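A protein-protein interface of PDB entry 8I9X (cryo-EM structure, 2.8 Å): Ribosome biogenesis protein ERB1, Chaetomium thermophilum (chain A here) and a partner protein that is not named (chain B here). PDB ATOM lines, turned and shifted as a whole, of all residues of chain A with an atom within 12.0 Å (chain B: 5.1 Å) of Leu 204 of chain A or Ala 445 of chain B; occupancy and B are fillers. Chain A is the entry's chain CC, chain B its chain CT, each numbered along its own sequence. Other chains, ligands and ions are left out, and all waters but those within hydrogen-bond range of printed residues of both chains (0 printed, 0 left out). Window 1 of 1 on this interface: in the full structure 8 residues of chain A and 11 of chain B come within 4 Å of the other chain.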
ATOM      1  N   THR A 200      18.008  10.840 -23.956  1.00  0.00           N
ATOM      2  CA  THR A 200      18.495  10.354 -22.674  1.00  0.00           C
ATOM      3  C   THR A 200      18.084   8.900 -22.482  1.00  0.00           C
ATOM      4  O   THR A 200      16.948   8.516 -22.780  1.00  0.00           O
ATOM      5  CB  THR A 200      17.979  11.224 -21.518  1.00  0.00           C
ATOM      6  OG1 THR A 200      18.564  10.784 -20.285  1.00  0.00           O
ATOM      7  CG2 THR A 200      16.456  11.177 -21.414  1.00  0.00           C
ATOM      8  N   GLY A 201      19.031   8.083 -22.024  1.00  0.00           N
ATOM      9  CA  GLY A 201      18.729   6.701 -21.732  1.00  0.00           C
ATOM     10  C   GLY A 201      18.007   6.535 -20.410  1.00  0.00           C
ATOM     11  O   GLY A 201      18.184   7.307 -19.469  1.00  0.00           O
ATOM     12  N   ASP A 202      17.175   5.502 -20.346  1.00  0.00           N
ATOM     13  CA  ASP A 202      16.427   5.227 -19.130  1.00  0.00           C
ATOM     14  C   ASP A 202      17.363   4.771 -18.017  1.00  0.00           C
ATOM     15  O   ASP A 202      18.340   4.052 -18.248  1.00  0.00           O
ATOM     16  CB  ASP A 202      15.362   4.163 -19.388  1.00  0.00           C
ATOM     17  CG  ASP A 202      14.246   4.661 -20.284  1.00  0.00           C
ATOM     18  OD1 ASP A 202      13.966   5.877 -20.268  1.00  0.00           O
ATOM     19  OD2 ASP A 202      13.648   3.834 -21.006  1.00  0.00           O
ATOM     20  N   ALA A 203      17.056   5.208 -16.793  1.00  0.00           N
ATOM     21  CA  ALA A 203      17.844   4.776 -15.645  1.00  0.00           C
ATOM     22  C   ALA A 203      17.756   3.271 -15.448  1.00  0.00           C
ATOM     23  O   ALA A 203      18.752   2.634 -15.088  1.00  0.00           O
ATOM     24  CB  ALA A 203      17.389   5.503 -14.382  1.00  0.00           C
ATOM     25  N   LEU A 204      16.579   2.687 -15.678  1.00  0.00           N
ATOM     26  CA  LEU A 204      16.460   1.237 -15.609  1.00  0.00           C
ATOM     27  C   LEU A 204      17.328   0.557 -16.658  1.00  0.00           C
ATOM     28  O   LEU A 204      17.976  -0.449 -16.358  1.00  0.00           O
ATOM     29  CB  LEU A 204      15.001   0.809 -15.769  1.00  0.00           C
ATOM     30  CG  LEU A 204      14.112   0.826 -14.524  1.00  0.00           C
ATOM     31  CD1 LEU A 204      14.652  -0.130 -13.476  1.00  0.00           C
ATOM     32  CD2 LEU A 204      13.974   2.225 -13.953  1.00  0.00           C
ATOM     33  N   GLN A 205      17.354   1.086 -17.883  1.00  0.00           N
ATOM     34  CA  GLN A 205      18.213   0.506 -18.909  1.00  0.00           C
ATOM     35  C   GLN A 205      19.682   0.605 -18.529  1.00  0.00           C
ATOM     36  O   GLN A 205      20.446  -0.340 -18.758  1.00  0.00           O
ATOM     37  CB  GLN A 205      17.962   1.187 -20.253  1.00  0.00           C
ATOM     38  CG  GLN A 205      18.518   0.443 -21.462  1.00  0.00           C
ATOM     39  CD  GLN A 205      18.210  -1.043 -21.448  1.00  0.00           C
ATOM     40  OE1 GLN A 205      18.910  -1.832 -20.813  1.00  0.00           O
ATOM     41  NE2 GLN A 205      17.153  -1.431 -22.151  1.00  0.00           N
ATOM     42  N   ASN A 206      20.097   1.732 -17.947  1.00  0.00           N
ATOM     43  CA  ASN A 206      21.470   1.850 -17.468  1.00  0.00           C
ATOM     44  C   ASN A 206      21.757   0.839 -16.364  1.00  0.00           C
ATOM     45  O   ASN A 206      22.854   0.273 -16.300  1.00  0.00           O
ATOM     46  CB  ASN A 206      21.735   3.272 -16.980  1.00  0.00           C
ATOM     47  CG  ASN A 206      21.791   4.274 -18.113  1.00  0.00           C
ATOM     48  OD1 ASN A 206      22.375   4.007 -19.162  1.00  0.00           O
ATOM     49  ND2 ASN A 206      21.180   5.434 -17.908  1.00  0.00           N
ATOM     50  N   LEU A 207      20.785   0.605 -15.481  1.00  0.00           N
ATOM     51  CA  LEU A 207      20.951  -0.408 -14.444  1.00  0.00           C
ATOM     52  C   LEU A 207      21.112  -1.803 -15.038  1.00  0.00           C
ATOM     53  O   LEU A 207      21.985  -2.561 -14.600  1.00  0.00           O
ATOM     54  CB  LEU A 207      19.768  -0.371 -13.479  1.00  0.00           C
ATOM     55  CG  LEU A 207      19.894   0.610 -12.313  1.00  0.00           C
ATOM     56  CD1 LEU A 207      18.553   0.817 -11.634  1.00  0.00           C
ATOM     57  CD2 LEU A 207      20.931   0.121 -11.319  1.00  0.00           C
ATOM     58  N   LEU A 208      20.288  -2.157 -16.027  1.00  0.00           N
ATOM     59  CA  LEU A 208      20.467  -3.441 -16.702  1.00  0.00           C
ATOM     60  C   LEU A 208      21.833  -3.531 -17.361  1.00  0.00           C
ATOM     61  O   LEU A 208      22.461  -4.594 -17.352  1.00  0.00           O
ATOM     62  CB  LEU A 208      19.382  -3.688 -17.756  1.00  0.00           C
ATOM     63  CG  LEU A 208      17.987  -4.242 -17.456  1.00  0.00           C
ATOM     64  CD1 LEU A 208      17.051  -3.217 -16.883  1.00  0.00           C
ATOM     65  CD2 LEU A 208      17.398  -4.846 -18.722  1.00  0.00           C
ATOM     66  N   ASP A 209      22.290  -2.442 -17.980  1.00  0.00           N
ATOM     67  CA  ASP A 209      23.596  -2.460 -18.625  1.00  0.00           C
ATOM     68  C   ASP A 209      24.707  -2.695 -17.610  1.00  0.00           C
ATOM     69  O   ASP A 209      25.618  -3.494 -17.859  1.00  0.00           O
ATOM     70  CB  ASP A 209      23.822  -1.150 -19.376  1.00  0.00           C
ATOM     71  CG  ASP A 209      23.081  -1.105 -20.698  1.00  0.00           C
ATOM     72  OD1 ASP A 209      23.143  -2.097 -21.450  1.00  0.00           O
ATOM     73  OD2 ASP A 209      22.437  -0.074 -20.984  1.00  0.00           O
ATOM     74  N   SER A 210      24.628  -2.031 -16.457  1.00  0.00           N
ATOM     75  CA  SER A 210      25.617  -2.231 -15.405  1.00  0.00           C
ATOM     76  C   SER A 210      25.583  -3.659 -14.873  1.00  0.00           C
ATOM     77  O   SER A 210      26.635  -4.244 -14.591  1.00  0.00           O
ATOM     78  CB  SER A 210      25.387  -1.231 -14.275  1.00  0.00           C
ATOM     79  OG  SER A 210      25.598   0.096 -14.722  1.00  0.00           O
ATOM     80  N   ILE A 211      24.391  -4.233 -14.719  1.00  0.00           N
ATOM     81  CA  ILE A 211      24.287  -5.610 -14.234  1.00  0.00           C
ATOM     82  C   ILE A 211      24.858  -6.584 -15.256  1.00  0.00           C
ATOM     83  O   ILE A 211      25.837  -7.289 -14.988  1.00  0.00           O
ATOM     84  CB  ILE A 211      22.828  -5.956 -13.888  1.00  0.00           C
ATOM     85  CG1 ILE A 211      22.303  -5.048 -12.777  1.00  0.00           C
ATOM     86  CG2 ILE A 211      22.714  -7.414 -13.476  1.00  0.00           C
ATOM     87  CD1 ILE A 211      23.055  -5.172 -11.484  1.00  0.00           C
ATOM     88  N   GLU A 212      24.256  -6.635 -16.440  1.00  0.00           N
ATOM     89  CA  GLU A 212      24.724  -7.476 -17.534  1.00  0.00           C
ATOM     90  C   GLU A 212      25.104  -6.581 -18.715  1.00  0.00           C
ATOM     91  O   GLU A 212      24.263  -6.238 -19.551  1.00  0.00           O
ATOM     92  CB  GLU A 212      23.666  -8.523 -17.895  1.00  0.00           C
ATOM     93  CG  GLU A 212      22.304  -7.989 -18.332  1.00  0.00           C
ATOM     94  CD  GLU A 212      21.305  -9.092 -18.614  1.00  0.00           C
ATOM     95  OE1 GLU A 212      21.660 -10.277 -18.443  1.00  0.00           O
ATOM     96  OE2 GLU A 212      20.163  -8.775 -19.009  1.00  0.00           O
ATOM     97  N   VAL A 213      26.372  -6.182 -18.754  1.00  0.00           N
ATOM     98  CA  VAL A 213      26.949  -5.349 -19.807  1.00  0.00           C
ATOM     99  C   VAL A 213      26.561  -5.856 -21.193  1.00  0.00           C
ATOM    100  O   VAL A 213      26.396  -7.069 -21.391  1.00  0.00           O
ATOM    101  CB  VAL A 213      28.477  -5.271 -19.659  1.00  0.00           C
ATOM    102  CG1 VAL A 213      28.850  -4.875 -18.241  1.00  0.00           C
ATOM    103  CG2 VAL A 213      29.122  -6.596 -20.026  1.00  0.00           C
ATOM    104  N   PRO A 214      26.384  -4.969 -22.165  1.00  0.00           N
ATOM    105  CA  PRO A 214      26.057  -5.410 -23.523  1.00  0.00           C
ATOM    106  C   PRO A 214      27.207  -6.194 -24.135  1.00  0.00           C
ATOM    107  O   PRO A 214      28.354  -6.138 -23.688  1.00  0.00           O
ATOM    108  CB  PRO A 214      25.809  -4.101 -24.280  1.00  0.00           C
ATOM    109  CG  PRO A 214      25.583  -3.075 -23.221  1.00  0.00           C
ATOM    110  CD  PRO A 214      26.411  -3.503 -22.056  1.00  0.00           C
ATOM    111  N   PHE B 409      14.856  -5.519 -12.406  1.00  0.00           N
ATOM    112  CA  PHE B 409      14.933  -4.363 -13.286  1.00  0.00           C
ATOM    113  C   PHE B 409      14.129  -4.560 -14.561  1.00  0.00           C
ATOM    114  O   PHE B 409      13.488  -3.615 -15.030  1.00  0.00           O
ATOM    115  CB  PHE B 409      16.391  -4.060 -13.623  1.00  0.00           C
ATOM    116  CG  PHE B 409      17.200  -3.576 -12.458  1.00  0.00           C
ATOM    117  CD1 PHE B 409      16.596  -2.927 -11.396  1.00  0.00           C
ATOM    118  CD2 PHE B 409      18.570  -3.762 -12.430  1.00  0.00           C
ATOM    119  CE1 PHE B 409      17.344  -2.480 -10.328  1.00  0.00           C
ATOM    120  CE2 PHE B 409      19.321  -3.317 -11.363  1.00  0.00           C
ATOM    121  CZ  PHE B 409      18.707  -2.674 -10.312  1.00  0.00           C
ATOM    122  N   LEU B 412      10.505  -4.066 -13.663  1.00  0.00           N
ATOM    123  CA  LEU B 412      10.232  -2.641 -13.493  1.00  0.00           C
ATOM    124  C   LEU B 412      10.160  -1.916 -14.829  1.00  0.00           C
ATOM    125  O   LEU B 412       9.298  -1.052 -15.017  1.00  0.00           O
ATOM    126  CB  LEU B 412      11.298  -1.997 -12.610  1.00  0.00           C
ATOM    127  CG  LEU B 412      11.150  -2.181 -11.103  1.00  0.00           C
ATOM    128  CD1 LEU B 412      12.190  -1.358 -10.373  1.00  0.00           C
ATOM    129  CD2 LEU B 412       9.751  -1.799 -10.656  1.00  0.00           C
ATOM    130  N   LYS B 413      11.050  -2.251 -15.762  1.00  0.00           N
ATOM    131  CA  LYS B 413      11.055  -1.575 -17.053  1.00  0.00           C
ATOM    132  C   LYS B 413       9.840  -1.965 -17.885  1.00  0.00           C
ATOM    133  O   LYS B 413       9.324  -1.149 -18.657  1.00  0.00           O
ATOM    134  CB  LYS B 413      12.351  -1.890 -17.796  1.00  0.00           C
ATOM    135  CG  LYS B 413      12.547  -1.103 -19.075  1.00  0.00           C
ATOM    136  CD  LYS B 413      13.978  -1.217 -19.571  1.00  0.00           C
ATOM    137  CE  LYS B 413      14.357  -2.660 -19.862  1.00  0.00           C
ATOM    138  NZ  LYS B 413      13.238  -3.435 -20.471  1.00  0.00           N
ATOM    139  N   GLY B 440      22.807   4.622  -5.488  1.00  0.00           N
ATOM    140  CA  GLY B 440      22.369   5.867  -6.102  1.00  0.00           C
ATOM    141  C   GLY B 440      21.553   5.671  -7.368  1.00  0.00           C
ATOM    142  O   GLY B 440      20.524   6.340  -7.552  1.00  0.00           O
ATOM    143  N   ASP B 441      21.985   4.754  -8.235  1.00  0.00           N
ATOM    144  CA  ASP B 441      21.261   4.481  -9.469  1.00  0.00           C
ATOM    145  C   ASP B 441      19.837   4.010  -9.213  1.00  0.00           C
ATOM    146  O   ASP B 441      18.928   4.438  -9.922  1.00  0.00           O
ATOM    147  CB  ASP B 441      22.012   3.442 -10.302  1.00  0.00           C
ATOM    148  CG  ASP B 441      23.419   3.884 -10.656  1.00  0.00           C
ATOM    149  OD1 ASP B 441      23.683   5.104 -10.637  1.00  0.00           O
ATOM    150  OD2 ASP B 441      24.261   3.011 -10.952  1.00  0.00           O
ATOM    151  N   LEU B 442      19.623   3.137  -8.229  1.00  0.00           N
ATOM    152  CA  LEU B 442      18.266   2.792  -7.817  1.00  0.00           C
ATOM    153  C   LEU B 442      17.487   3.981  -7.274  1.00  0.00           C
ATOM    154  O   LEU B 442      16.272   4.053  -7.492  1.00  0.00           O
ATOM    155  CB  LEU B 442      18.266   1.666  -6.776  1.00  0.00           C
ATOM    156  CG  LEU B 442      18.369   0.202  -7.231  1.00  0.00           C
ATOM    157  CD1 LEU B 442      19.722  -0.200  -7.775  1.00  0.00           C
ATOM    158  CD2 LEU B 442      17.974  -0.715  -6.081  1.00  0.00           C
ATOM    159  N   LEU B 443      18.141   4.912  -6.576  1.00  0.00           N
ATOM    160  CA  LEU B 443      17.397   6.099  -6.152  1.00  0.00           C
ATOM    161  C   LEU B 443      16.847   6.882  -7.342  1.00  0.00           C
ATOM    162  O   LEU B 443      15.649   7.200  -7.383  1.00  0.00           O
ATOM    163  CB  LEU B 443      18.264   7.001  -5.276  1.00  0.00           C
ATOM    164  CG  LEU B 443      18.164   6.715  -3.778  1.00  0.00           C
ATOM    165  CD1 LEU B 443      18.821   7.823  -2.981  1.00  0.00           C
ATOM    166  CD2 LEU B 443      16.713   6.546  -3.368  1.00  0.00           C
ATOM    167  N   GLU B 444      17.685   7.186  -8.335  1.00  0.00           N
ATOM    168  CA  GLU B 444      17.128   7.877  -9.505  1.00  0.00           C
ATOM    169  C   GLU B 444      16.261   6.975 -10.383  1.00  0.00           C
ATOM    170  O   GLU B 444      15.425   7.483 -11.137  1.00  0.00           O
ATOM    171  CB  GLU B 444      18.204   8.584 -10.335  1.00  0.00           C
ATOM    172  CG  GLU B 444      18.695   9.903  -9.724  1.00  0.00           C
ATOM    173  CD  GLU B 444      19.744   9.769  -8.662  1.00  0.00           C
ATOM    174  OE1 GLU B 444      20.195   8.646  -8.408  1.00  0.00           O
ATOM    175  OE2 GLU B 444      20.102  10.801  -8.057  1.00  0.00           O
ATOM    176  N   ALA B 445      16.393   5.654 -10.279  1.00  0.00           N
ATOM    177  CA  ALA B 445      15.430   4.784 -10.948  1.00  0.00           C
ATOM    178  C   ALA B 445      14.042   4.939 -10.340  1.00  0.00           C
ATOM    179  O   ALA B 445      13.041   5.017 -11.062  1.00  0.00           O
ATOM    180  CB  ALA B 445      15.891   3.329 -10.876  1.00  0.00           C
ATOM    181  N   LEU B 446      13.966   4.995  -9.011  1.00  0.00           N
ATOM    182  CA  LEU B 446      12.694   5.263  -8.350  1.00  0.00           C
ATOM    183  C   LEU B 446      12.172   6.646  -8.717  1.00  0.00           C
ATOM    184  O   LEU B 446      10.962   6.835  -8.903  1.00  0.00           O
ATOM    185  CB  LEU B 446      12.856   5.130  -6.839  1.00  0.00           C
ATOM    186  CG  LEU B 446      12.920   3.700  -6.312  1.00  0.00           C
ATOM    187  CD1 LEU B 446      13.369   3.689  -4.864  1.00  0.00           C
ATOM    188  CD2 LEU B 446      11.574   3.015  -6.464  1.00  0.00           C
ATOM    189  N   LYS B 447      13.073   7.624  -8.821  1.00  0.00           N
ATOM    190  CA  LYS B 447      12.672   8.950  -9.284  1.00  0.00           C
ATOM    191  C   LYS B 447      12.037   8.886 -10.670  1.00  0.00           C
ATOM    192  O   LYS B 447      11.006   9.526 -10.916  1.00  0.00           O
ATOM    193  CB  LYS B 447      13.884   9.877  -9.309  1.00  0.00           C
ATOM    194  CG  LYS B 447      14.099  10.685  -8.049  1.00  0.00           C
ATOM    195  CD  LYS B 447      15.293  11.609  -8.212  1.00  0.00           C
ATOM    196  CE  LYS B 447      15.691  12.247  -6.898  1.00  0.00           C
ATOM    197  NZ  LYS B 447      16.739  11.452  -6.206  1.00  0.00           N
ATOM    198  N   ASP B 448      12.638   8.118 -11.581  1.00  0.00           N
ATOM    199  CA  ASP B 448      12.089   7.959 -12.922  1.00  0.00           C
ATOM    200  C   ASP B 448      10.744   7.249 -12.916  1.00  0.00           C
ATOM    201  O   ASP B 448       9.866   7.604 -13.706  1.00  0.00           O
ATOM    202  CB  ASP B 448      13.070   7.198 -13.811  1.00  0.00           C
ATOM    203  CG  ASP B 448      14.168   8.084 -14.350  1.00  0.00           C
ATOM    204  OD1 ASP B 448      14.117   9.307 -14.107  1.00  0.00           O
ATOM    205  OD2 ASP B 448      15.076   7.562 -15.028  1.00  0.00           O
ATOM    206  N   LEU B 449      10.566   6.242 -12.062  1.00  0.00           N
ATOM    207  CA  LEU B 449       9.241   5.638 -11.930  1.00  0.00           C
ATOM    208  C   LEU B 449       8.201   6.643 -11.449  1.00  0.00           C
ATOM    209  O   LEU B 449       7.083   6.670 -11.981  1.00  0.00           O
ATOM    210  CB  LEU B 449       9.276   4.432 -10.989  1.00  0.00           C
ATOM    211  CG  LEU B 449       9.645   3.049 -11.540  1.00  0.00           C
ATOM    212  CD1 LEU B 449       8.597   2.589 -12.535  1.00  0.00           C
ATOM    213  CD2 LEU B 449      11.010   3.020 -12.180  1.00  0.00           C
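Along chain A the printed residues that touch a printed residue of chain B span positions 203 to 211. Of the 13 printed residues of chain B, 8 touch a printed residue of chain A. Along chain B the printed residues that touch a printed residue of chain A span positions 409 to 449. Among the printed residues, no Asp or Glu carboxylate lies within 4 Å of a Lys or Arg side-chain nitrogen of the other chain.
Of the printed residues of chain B, Leu 204 of chain A touches Phe 409, Leu 412, Ala 445 and Leu 449. Of chain A, only Leu 204 comes within 4 Å of Leu 412 of chain B. Leu 442 of chain B touches just one residue of chain A: Leu 207 (3.8 Å). No residue of chain A comes within 4 Å of Glu 444 of chain B. No residue of chain A comes within 4 Å of Leu 446 of chain B. Asp 448 of chain B touches one residue of chain A. Leu 449 of chain B touches just one residue of chain A: Leu 204 (3.5 Å). Of the printed residues of chain A, Phe 409 of chain B touches Leu 204 (3.99 Å), Leu 207 (3.7 Å), Leu 208 (3.4 Å) and Ile 211 (3.7 Å). Printed residues of chain B within 4 Å of Leu 207 of chain A: Phe 409, Asp 441, Leu 442 and Ala 445. Printed residues of chain B within 4 Å of Leu 208 of chain A: Phe 409 and Lys 413. Val 213 of chain A touches none of the printed residues of chain B. The nearest printed residue of chain B that does not touch Leu 204 of chain A is Lys 413 of chain B (4.3 Å). The nearest printed residue of chain A that does not touch Ala 445 of chain B is Ala 203 of chain A (4.02 Å). The nearest printed residue of chain B that does not touch Ile 211 of chain A is Leu 442 of chain B (7.0 Å).
Ala 203 of chain A touches Asp 448 of chain B. Leu 204 of chain A touches Leu 412 of chain B (CD1 to CB, 3.9 Å). CD2 of Leu 204 of chain A touches CB of Ala 445 of chain B, at 3.8 Å. Leu 449 of chain B touches Leu 204 of chain A (CD2 to CD2, 3.5 Å). Gln 205 of chain A touches Lys 413 of chain B (NE2 to CE, 3.8 Å). Leu 207 of chain A touches Phe 409 of chain B. CD1 of Leu 207 of chain A touches CB of Ala 445 of chain B, 3.7 Å away. Leu 208 of chain A touches Phe 409 of chain B. CD2 of Leu 208 of chain A touches CE of Lys 413 of chain B, at 3.9 Å. Ile 211 of chain A touches Phe 409 of chain B (CG1 to CE2, 3.7 Å).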
